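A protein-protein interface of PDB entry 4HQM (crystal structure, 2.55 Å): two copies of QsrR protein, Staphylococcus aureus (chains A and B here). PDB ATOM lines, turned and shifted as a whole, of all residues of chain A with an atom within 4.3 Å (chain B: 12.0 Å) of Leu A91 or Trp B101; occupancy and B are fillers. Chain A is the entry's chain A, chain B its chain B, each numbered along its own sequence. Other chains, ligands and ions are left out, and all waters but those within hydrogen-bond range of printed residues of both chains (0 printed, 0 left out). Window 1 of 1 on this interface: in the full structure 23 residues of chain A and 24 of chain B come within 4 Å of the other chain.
The indole nitrogen (NE1) of Trp B101 sits at hydrogen-bond distance from the backbone carbonyl oxygen (O) of Lys A87 (3.3 Å).
OG1 of Thr A14 lies within hydrogen-bond range of O of Tyr A10 (2.8 Å). NZ of Lys A87 sits at hydrogen-bond distance from OH of Tyr A10 (2.5 Å).
Among the printed residues, pairs that only touch across the chains: Lys A87 with Tyr B105 (3.2 Å), Ala A90 with Tyr B105 (3.4 Å), Leu A91 with Trp B101 (3.6 Å), Ala A90 with Trp B101 (3.6 Å), Leu A91 with Ile B98 (3.6 Å), Thr A14 with Trp B101 (3.8 Å), Leu A95 with Ile B98 (3.8 Å), Ala A94 with Ile B98 (3.9 Å) and Tyr A10 with Trp B101 (3.98 Å).
Of chain B, only Ile B98 (3.6 Å) and Trp B101 (3.6 Å) come within 4 Å of Leu A91. Trp B101 touches just these residues of chain A: Tyr A10 (3.98 Å), Thr A14 (3.8 Å), Lys A87 (3.3 Å), Ala A90 (3.6 Å) and Leu A91 (3.6 Å). Of chain B, only Trp B101 comes within 4 Å of Thr A14. Lys A87 touches two residues of chain B. Gly A88 touches none of the printed residues of chain B. Of chain B, only Trp B101 and Tyr B105 come within 4 Å of Ala A90. Ala A92 touches none of the printed residues of chain B. Printed residues of chain B within 4 Å of Leu A95: Ile B98. Of the printed residues of chain B, Tyr A10 touches Trp B101 (3.98 Å). Of the printed residues of chain A, Ile B98 touches Leu A91 (3.6 Å), Ala A94 (3.9 Å) and Leu A95 (3.8 Å). The nearest residue of chain B that does not touch Leu A91 is Tyr B105 (5.7 Å). The nearest printed residue of chain A that does not touch Trp B101 is Ala A94 (4.4 Å). The nearest printed residue of chain A that does not touch Tyr B105 is Tyr A10 (4.5 Å).
Hydrophobic or aromatic side chains of chain A within 4 Å of the printed part of chain B: Tyr A10, Ala A90, Leu A91, Ala A94 and Leu A95. Of the 19 printed residues of chain B, 3 touch a printed residue of chain A. Hydrophobic or aromatic side chains of chain B that line the printed part of chain A: Ile B98, Trp B101 and Tyr B105. Among the printed residues, 10 pairs touch across the chains. Among the printed residues, no Asp or Glu carboxylate lies within 4 Å of a Lys or Arg side-chain nitrogen of the other chain.
4 positions are printed for both chains.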
ATOM      1  N   TYR A  10      15.517  13.713 -15.928  1.00  0.00           N
ATOM      2  CA  TYR A  10      16.084  15.029 -16.168  1.00  0.00           C
ATOM      3  C   TYR A  10      16.239  15.185 -17.681  1.00  0.00           C
ATOM      4  O   TYR A  10      15.714  16.115 -18.281  1.00  0.00           O
ATOM      5  CB  TYR A  10      17.419  15.247 -15.432  1.00  0.00           C
ATOM      6  CG  TYR A  10      17.774  16.700 -15.167  1.00  0.00           C
ATOM      7  CD1 TYR A  10      17.096  17.440 -14.201  1.00  0.00           C
ATOM      8  CD2 TYR A  10      18.777  17.338 -15.895  1.00  0.00           C
ATOM      9  CE1 TYR A  10      17.410  18.779 -13.961  1.00  0.00           C
ATOM     10  CE2 TYR A  10      19.103  18.675 -15.660  1.00  0.00           C
ATOM     11  CZ  TYR A  10      18.413  19.390 -14.693  1.00  0.00           C
ATOM     12  OH  TYR A  10      18.722  20.714 -14.462  1.00  0.00           O
ATOM     13  N   THR A  14      14.287  17.714 -19.874  1.00  0.00           N
ATOM     14  CA  THR A  14      14.983  18.630 -20.705  1.00  0.00           C
ATOM     15  C   THR A  14      14.469  18.584 -22.132  1.00  0.00           C
ATOM     16  O   THR A  14      14.133  19.575 -22.710  1.00  0.00           O
ATOM     17  CB  THR A  14      16.472  18.272 -20.731  1.00  0.00           C
ATOM     18  OG1 THR A  14      16.988  18.259 -19.447  1.00  0.00           O
ATOM     19  CG2 THR A  14      17.289  19.262 -21.511  1.00  0.00           C
ATOM     20  N   LEU A  67      18.625  27.715 -17.317  1.00  0.00           N
ATOM     21  CA  LEU A  67      19.365  27.704 -18.545  1.00  0.00           C
ATOM     22  C   LEU A  67      19.647  29.136 -18.960  1.00  0.00           C
ATOM     23  O   LEU A  67      20.684  29.434 -19.485  1.00  0.00           O
ATOM     24  CB  LEU A  67      18.561  27.016 -19.633  1.00  0.00           C
ATOM     25  CG  LEU A  67      18.163  25.579 -19.342  1.00  0.00           C
ATOM     26  CD1 LEU A  67      17.320  25.006 -20.450  1.00  0.00           C
ATOM     27  CD2 LEU A  67      19.350  24.694 -19.156  1.00  0.00           C
ATOM     28  N   LYS A  87      25.114  26.095 -17.239  1.00  0.00           N
ATOM     29  CA  LYS A  87      24.303  24.966 -17.586  1.00  0.00           C
ATOM     30  C   LYS A  87      23.658  25.118 -18.936  1.00  0.00           C
ATOM     31  O   LYS A  87      23.699  24.243 -19.753  1.00  0.00           O
ATOM     32  CB  LYS A  87      23.248  24.770 -16.538  1.00  0.00           C
ATOM     33  CG  LYS A  87      22.920  23.315 -16.378  1.00  0.00           C
ATOM     34  CD  LYS A  87      21.461  22.977 -16.364  1.00  0.00           C
ATOM     35  CE  LYS A  87      20.818  23.264 -15.042  1.00  0.00           C
ATOM     36  NZ  LYS A  87      19.405  22.992 -15.186  1.00  0.00           N
ATOM     37  N   GLY A  88      23.173  26.290 -19.229  1.00  0.00           N
ATOM     38  CA  GLY A  88      22.651  26.519 -20.534  1.00  0.00           C
ATOM     39  C   GLY A  88      23.661  26.426 -21.648  1.00  0.00           C
ATOM     40  O   GLY A  88      23.397  25.843 -22.676  1.00  0.00           O
ATOM     41  N   LYS A  89      24.821  27.024 -21.449  1.00  0.00           N
ATOM     42  CA  LYS A  89      25.886  27.036 -22.431  1.00  0.00           C
ATOM     43  C   LYS A  89      26.392  25.617 -22.701  1.00  0.00           C
ATOM     44  O   LYS A  89      26.607  25.188 -23.828  1.00  0.00           O
ATOM     45  CB  LYS A  89      27.002  27.996 -21.993  1.00  0.00           C
ATOM     46  CG  LYS A  89      26.840  29.475 -22.417  1.00  0.00           C
ATOM     47  CD  LYS A  89      28.106  30.343 -22.295  1.00  0.00           C
ATOM     48  CE  LYS A  89      28.787  30.255 -20.922  1.00  0.00           C
ATOM     49  NZ  LYS A  89      29.968  31.143 -20.865  1.00  0.00           N
ATOM     50  N   ALA A  90      26.524  24.877 -21.625  1.00  0.00           N
ATOM     51  CA  ALA A  90      26.904  23.512 -21.683  1.00  0.00           C
ATOM     52  C   ALA A  90      25.891  22.678 -22.448  1.00  0.00           C
ATOM     53  O   ALA A  90      26.233  21.872 -23.286  1.00  0.00           O
ATOM     54  CB  ALA A  90      27.100  23.056 -20.295  1.00  0.00           C
ATOM     55  N   LEU A  91      24.623  22.948 -22.228  1.00  0.00           N
ATOM     56  CA  LEU A  91      23.582  22.335 -23.014  1.00  0.00           C
ATOM     57  C   LEU A  91      23.695  22.609 -24.472  1.00  0.00           C
ATOM     58  O   LEU A  91      23.539  21.720 -25.257  1.00  0.00           O
ATOM     59  CB  LEU A  91      22.212  22.741 -22.505  1.00  0.00           C
ATOM     60  CG  LEU A  91      21.031  22.156 -23.256  1.00  0.00           C
ATOM     61  CD1 LEU A  91      21.008  20.664 -23.257  1.00  0.00           C
ATOM     62  CD2 LEU A  91      19.756  22.692 -22.676  1.00  0.00           C
ATOM     63  N   ALA A  92      23.927  23.840 -24.831  1.00  0.00           N
ATOM     64  CA  ALA A  92      23.993  24.233 -26.224  1.00  0.00           C
ATOM     65  C   ALA A  92      25.071  23.477 -26.990  1.00  0.00           C
ATOM     66  O   ALA A  92      24.877  22.954 -28.083  1.00  0.00           O
ATOM     67  CB  ALA A  92      24.237  25.707 -26.283  1.00  0.00           C
ATOM     68  N   GLU A  93      26.202  23.365 -26.317  1.00  0.00           N
ATOM     69  CA  GLU A  93      27.293  22.552 -26.768  1.00  0.00           C
ATOM     70  C   GLU A  93      26.844  21.099 -26.985  1.00  0.00           C
ATOM     71  O   GLU A  93      27.128  20.485 -27.998  1.00  0.00           O
ATOM     72  CB  GLU A  93      28.439  22.627 -25.764  1.00  0.00           C
ATOM     73  CG  GLU A  93      29.239  23.926 -25.838  1.00  0.00           C
ATOM     74  CD  GLU A  93      30.210  24.027 -27.015  1.00  0.00           C
ATOM     75  OE1 GLU A  93      30.407  23.031 -27.745  1.00  0.00           O
ATOM     76  OE2 GLU A  93      30.803  25.125 -27.193  1.00  0.00           O
ATOM     77  N   ALA A  94      26.115  20.583 -25.997  1.00  0.00           N
ATOM     78  CA  ALA A  94      25.617  19.225 -25.986  1.00  0.00           C
ATOM     79  C   ALA A  94      24.666  18.952 -27.133  1.00  0.00           C
ATOM     80  O   ALA A  94      24.678  17.901 -27.717  1.00  0.00           O
ATOM     81  CB  ALA A  94      25.009  18.911 -24.657  1.00  0.00           C
ATOM     82  N   LEU A  95      23.839  19.921 -27.458  1.00  0.00           N
ATOM     83  CA  LEU A  95      22.948  19.838 -28.596  1.00  0.00           C
ATOM     84  C   LEU A  95      23.638  19.667 -29.937  1.00  0.00           C
ATOM     85  O   LEU A  95      23.104  19.024 -30.811  1.00  0.00           O
ATOM     86  CB  LEU A  95      21.989  20.994 -28.649  1.00  0.00           C
ATOM     87  CG  LEU A  95      21.078  21.033 -27.427  1.00  0.00           C
ATOM     88  CD1 LEU A  95      20.051  22.134 -27.548  1.00  0.00           C
ATOM     89  CD2 LEU A  95      20.362  19.731 -27.081  1.00  0.00           C
ATOM     90  N   LEU B  11      14.456  18.588 -35.429  1.00  0.00           N
ATOM     91  CA  LEU B  11      14.993  18.601 -34.106  1.00  0.00           C
ATOM     92  C   LEU B  11      13.917  18.800 -33.059  1.00  0.00           C
ATOM     93  O   LEU B  11      13.901  18.099 -32.077  1.00  0.00           O
ATOM     94  CB  LEU B  11      15.945  19.775 -33.987  1.00  0.00           C
ATOM     95  CG  LEU B  11      17.319  19.483 -34.513  1.00  0.00           C
ATOM     96  CD1 LEU B  11      18.037  20.785 -34.785  1.00  0.00           C
ATOM     97  CD2 LEU B  11      18.060  18.620 -33.503  1.00  0.00           C
ATOM     98  N   PHE B  15      13.131  15.990 -30.267  1.00  0.00           N
ATOM     99  CA  PHE B  15      13.095  16.399 -28.896  1.00  0.00           C
ATOM    100  C   PHE B  15      11.838  15.969 -28.236  1.00  0.00           C
ATOM    101  O   PHE B  15      11.827  15.436 -27.178  1.00  0.00           O
ATOM    102  CB  PHE B  15      13.276  17.890 -28.776  1.00  0.00           C
ATOM    103  CG  PHE B  15      14.594  18.403 -29.175  1.00  0.00           C
ATOM    104  CD1 PHE B  15      15.768  17.693 -29.040  1.00  0.00           C
ATOM    105  CD2 PHE B  15      14.677  19.727 -29.594  1.00  0.00           C
ATOM    106  CE1 PHE B  15      16.985  18.297 -29.292  1.00  0.00           C
ATOM    107  CE2 PHE B  15      15.892  20.355 -29.842  1.00  0.00           C
ATOM    108  CZ  PHE B  15      17.047  19.626 -29.686  1.00  0.00           C
ATOM    109  N   LEU B  18      11.644  12.499 -27.630  1.00  0.00           N
ATOM    110  CA  LEU B  18      12.612  12.213 -26.585  1.00  0.00           C
ATOM    111  C   LEU B  18      12.125  12.616 -25.222  1.00  0.00           C
ATOM    112  O   LEU B  18      12.356  11.936 -24.262  1.00  0.00           O
ATOM    113  CB  LEU B  18      13.936  12.808 -26.879  1.00  0.00           C
ATOM    114  CG  LEU B  18      14.581  12.111 -28.043  1.00  0.00           C
ATOM    115  CD1 LEU B  18      15.854  12.809 -28.434  1.00  0.00           C
ATOM    116  CD2 LEU B  18      14.878  10.672 -27.741  1.00  0.00           C
ATOM    117  N   GLY B  19      11.392  13.693 -25.193  1.00  0.00           N
ATOM    118  CA  GLY B  19      10.657  14.223 -24.089  1.00  0.00           C
ATOM    119  C   GLY B  19       9.685  13.300 -23.475  1.00  0.00           C
ATOM    120  O   GLY B  19       9.591  13.236 -22.277  1.00  0.00           O
ATOM    121  N   ALA B  92      21.461   7.625 -31.104  1.00  0.00           N
ATOM    122  CA  ALA B  92      22.074   7.168 -29.860  1.00  0.00           C
ATOM    123  C   ALA B  92      23.507   7.704 -29.716  1.00  0.00           C
ATOM    124  O   ALA B  92      23.953   8.082 -28.650  1.00  0.00           O
ATOM    125  CB  ALA B  92      22.033   5.654 -29.780  1.00  0.00           C
ATOM    126  N   GLU B  93      24.216   7.723 -30.829  1.00  0.00           N
ATOM    127  CA  GLU B  93      25.580   8.230 -30.862  1.00  0.00           C
ATOM    128  C   GLU B  93      25.654   9.732 -30.539  1.00  0.00           C
ATOM    129  O   GLU B  93      26.510  10.192 -29.771  1.00  0.00           O
ATOM    130  CB  GLU B  93      26.243   7.970 -32.213  1.00  0.00           C
ATOM    131  CG  GLU B  93      27.666   7.437 -32.077  1.00  0.00           C
ATOM    132  CD  GLU B  93      27.625   6.046 -31.482  1.00  0.00           C
ATOM    133  OE1 GLU B  93      27.581   5.095 -32.282  1.00  0.00           O
ATOM    134  OE2 GLU B  93      27.632   5.887 -30.245  1.00  0.00           O
ATOM    135  N   ALA B  94      24.706  10.478 -31.124  1.00  0.00           N
ATOM    136  CA  ALA B  94      24.541  11.904 -30.892  1.00  0.00           C
ATOM    137  C   ALA B  94      24.099  12.209 -29.462  1.00  0.00           C
ATOM    138  O   ALA B  94      24.445  13.221 -28.896  1.00  0.00           O
ATOM    139  CB  ALA B  94      23.527  12.454 -31.852  1.00  0.00           C
ATOM    140  N   LEU B  95      23.310  11.321 -28.891  1.00  0.00           N
ATOM    141  CA  LEU B  95      22.836  11.448 -27.533  1.00  0.00           C
ATOM    142  C   LEU B  95      23.921  11.551 -26.480  1.00  0.00           C
ATOM    143  O   LEU B  95      23.717  12.198 -25.482  1.00  0.00           O
ATOM    144  CB  LEU B  95      21.832  10.372 -27.194  1.00  0.00           C
ATOM    145  CG  LEU B  95      20.369  10.850 -27.143  1.00  0.00           C
ATOM    146  CD1 LEU B  95      19.989  11.481 -25.792  1.00  0.00           C
ATOM    147  CD2 LEU B  95      19.982  11.759 -28.292  1.00  0.00           C
ATOM    148  N   HIS B  96      24.959  10.730 -26.585  1.00  0.00           N
ATOM    149  CA  HIS B  96      25.983  10.627 -25.522  1.00  0.00           C
ATOM    150  C   HIS B  96      26.402  11.959 -24.805  1.00  0.00           C
ATOM    151  O   HIS B  96      26.459  12.011 -23.585  1.00  0.00           O
ATOM    152  CB  HIS B  96      27.235   9.899 -26.046  1.00  0.00           C
ATOM    153  CG  HIS B  96      26.985   8.468 -26.389  1.00  0.00           C
ATOM    154  ND1 HIS B  96      27.263   7.881 -27.594  1.00  0.00           N
ATOM    155  CD2 HIS B  96      26.467   7.488 -25.623  1.00  0.00           C
ATOM    156  CE1 HIS B  96      26.889   6.603 -27.500  1.00  0.00           C
ATOM    157  NE2 HIS B  96      26.399   6.317 -26.331  1.00  0.00           N
ATOM    158  N   PRO B  97      26.712  13.080 -25.455  1.00  0.00           N
ATOM    159  CA  PRO B  97      27.123  14.277 -24.741  1.00  0.00           C
ATOM    160  C   PRO B  97      26.047  14.877 -23.851  1.00  0.00           C
ATOM    161  O   PRO B  97      26.361  15.304 -22.752  1.00  0.00           O
ATOM    162  CB  PRO B  97      27.564  15.191 -25.823  1.00  0.00           C
ATOM    163  CG  PRO B  97      27.328  14.489 -27.137  1.00  0.00           C
ATOM    164  CD  PRO B  97      27.225  13.066 -26.771  1.00  0.00           C
ATOM    165  N   ILE B  98      24.796  14.871 -24.292  1.00  0.00           N
ATOM    166  CA  ILE B  98      23.728  15.416 -23.475  1.00  0.00           C
ATOM    167  C   ILE B  98      23.421  14.498 -22.307  1.00  0.00           C
ATOM    168  O   ILE B  98      23.075  14.912 -21.218  1.00  0.00           O
ATOM    169  CB  ILE B  98      22.492  15.863 -24.268  1.00  0.00           C
ATOM    170  CG1 ILE B  98      21.385  16.445 -23.404  1.00  0.00           C
ATOM    171  CG2 ILE B  98      22.026  14.791 -25.182  1.00  0.00           C
ATOM    172  CD1 ILE B  98      20.322  17.219 -24.191  1.00  0.00           C
ATOM    173  N   GLU B  99      23.670  13.222 -22.513  1.00  0.00           N
ATOM    174  CA  GLU B  99      23.547  12.269 -21.445  1.00  0.00           C
ATOM    175  C   GLU B  99      24.566  12.544 -20.347  1.00  0.00           C
ATOM    176  O   GLU B  99      24.270  12.537 -19.161  1.00  0.00           O
ATOM    177  CB  GLU B  99      23.767  10.876 -22.008  1.00  0.00           C
ATOM    178  CG  GLU B  99      23.373   9.761 -21.057  1.00  0.00           C
ATOM    179  CD  GLU B  99      23.845   8.422 -21.581  1.00  0.00           C
ATOM    180  OE1 GLU B  99      23.647   7.421 -20.851  1.00  0.00           O
ATOM    181  OE2 GLU B  99      24.402   8.354 -22.699  1.00  0.00           O
ATOM    182  N   ALA B 100      25.784  12.817 -20.788  1.00  0.00           N
ATOM    183  CA  ALA B 100      26.873  13.156 -19.891  1.00  0.00           C
ATOM    184  C   ALA B 100      26.606  14.432 -19.103  1.00  0.00           C
ATOM    185  O   ALA B 100      26.735  14.506 -17.880  1.00  0.00           O
ATOM    186  CB  ALA B 100      28.124  13.356 -20.719  1.00  0.00           C
ATOM    187  N   TRP B 101      26.171  15.448 -19.842  1.00  0.00           N
ATOM    188  CA  TRP B 101      25.783  16.730 -19.285  1.00  0.00           C
ATOM    189  C   TRP B 101      24.726  16.595 -18.223  1.00  0.00           C
ATOM    190  O   TRP B 101      24.799  17.244 -17.160  1.00  0.00           O
ATOM    191  CB  TRP B 101      25.289  17.638 -20.409  1.00  0.00           C
ATOM    192  CG  TRP B 101      24.536  18.868 -19.954  1.00  0.00           C
ATOM    193  CD1 TRP B 101      25.058  20.125 -19.671  1.00  0.00           C
ATOM    194  CD2 TRP B 101      23.089  19.002 -19.737  1.00  0.00           C
ATOM    195  NE1 TRP B 101      24.067  20.994 -19.296  1.00  0.00           N
ATOM    196  CE2 TRP B 101      22.865  20.385 -19.315  1.00  0.00           C
ATOM    197  CE3 TRP B 101      22.003  18.149 -19.839  1.00  0.00           C
ATOM    198  CZ2 TRP B 101      21.605  20.865 -19.015  1.00  0.00           C
ATOM    199  CZ3 TRP B 101      20.736  18.646 -19.533  1.00  0.00           C
ATOM    200  CH2 TRP B 101      20.543  19.971 -19.132  1.00  0.00           C
ATOM    201  N   ALA B 102      23.730  15.757 -18.491  1.00  0.00           N
ATOM    202  CA  ALA B 102      22.618  15.564 -17.605  1.00  0.00           C
ATOM    203  C   ALA B 102      23.096  15.063 -16.275  1.00  0.00           C
ATOM    204  O   ALA B 102      22.700  15.565 -15.235  1.00  0.00           O
ATOM    205  CB  ALA B 102      21.628  14.589 -18.207  1.00  0.00           C
ATOM    206  N   GLN B 103      24.033  14.125 -16.326  1.00  0.00           N
ATOM    207  CA  GLN B 103      24.638  13.655 -15.102  1.00  0.00           C
ATOM    208  C   GLN B 103      25.398  14.766 -14.346  1.00  0.00           C
ATOM    209  O   GLN B 103      25.304  14.839 -13.124  1.00  0.00           O
ATOM    210  CB  GLN B 103      25.559  12.455 -15.324  1.00  0.00           C
ATOM    211  CG  GLN B 103      26.108  11.858 -14.017  1.00  0.00           C
ATOM    212  CD  GLN B 103      25.025  11.448 -13.016  1.00  0.00           C
ATOM    213  OE1 GLN B 103      24.433  10.358 -13.119  1.00  0.00           O
ATOM    214  NE2 GLN B 103      24.774  12.326 -12.001  1.00  0.00           N
ATOM    215  N   SER B 104      26.153  15.642 -15.026  1.00  0.00           N
ATOM    216  CA  SER B 104      26.831  16.675 -14.232  1.00  0.00           C
ATOM    217  C   SER B 104      25.873  17.523 -13.371  1.00  0.00           C
ATOM    218  O   SER B 104      26.044  17.602 -12.167  1.00  0.00           O
ATOM    219  CB  SER B 104      27.549  17.671 -15.128  1.00  0.00           C
ATOM    220  OG  SER B 104      28.458  17.024 -15.982  1.00  0.00           O
ATOM    221  N   TYR B 105      24.792  18.033 -13.956  1.00  0.00           N
ATOM    222  CA  TYR B 105      23.867  18.918 -13.225  1.00  0.00           C
ATOM    223  C   TYR B 105      22.795  18.321 -12.274  1.00  0.00           C
ATOM    224  O   TYR B 105      22.473  18.936 -11.260  1.00  0.00           O
ATOM    225  CB  TYR B 105      23.213  19.905 -14.197  1.00  0.00           C
ATOM    226  CG  TYR B 105      24.216  20.766 -14.928  1.00  0.00           C
ATOM    227  CD1 TYR B 105      24.811  21.853 -14.303  1.00  0.00           C
ATOM    228  CD2 TYR B 105      24.582  20.481 -16.235  1.00  0.00           C
ATOM    229  CE1 TYR B 105      25.735  22.638 -14.964  1.00  0.00           C
ATOM    230  CE2 TYR B 105      25.506  21.260 -16.903  1.00  0.00           C
ATOM    231  CZ  TYR B 105      26.079  22.338 -16.263  1.00  0.00           C
ATOM    232  OH  TYR B 105      26.998  23.115 -16.928  1.00  0.00           O
ATOM    233  N   VAL B 106      22.238  17.155 -12.594  1.00  0.00           N
ATOM    234  CA  VAL B 106      21.128  16.565 -11.817  1.00  0.00           C
ATOM    235  C   VAL B 106      20.614  17.151 -10.493  1.00  0.00           C
ATOM    236  O   VAL B 106      19.412  17.499 -10.426  1.00  0.00           O
ATOM    237  CB  VAL B 106      21.465  15.126 -11.414  1.00  0.00           C
ATOM    238  CG1 VAL B 106      21.484  14.279 -12.676  1.00  0.00           C
ATOM    239  CG2 VAL B 106      22.847  15.031 -10.749  1.00  0.00           C
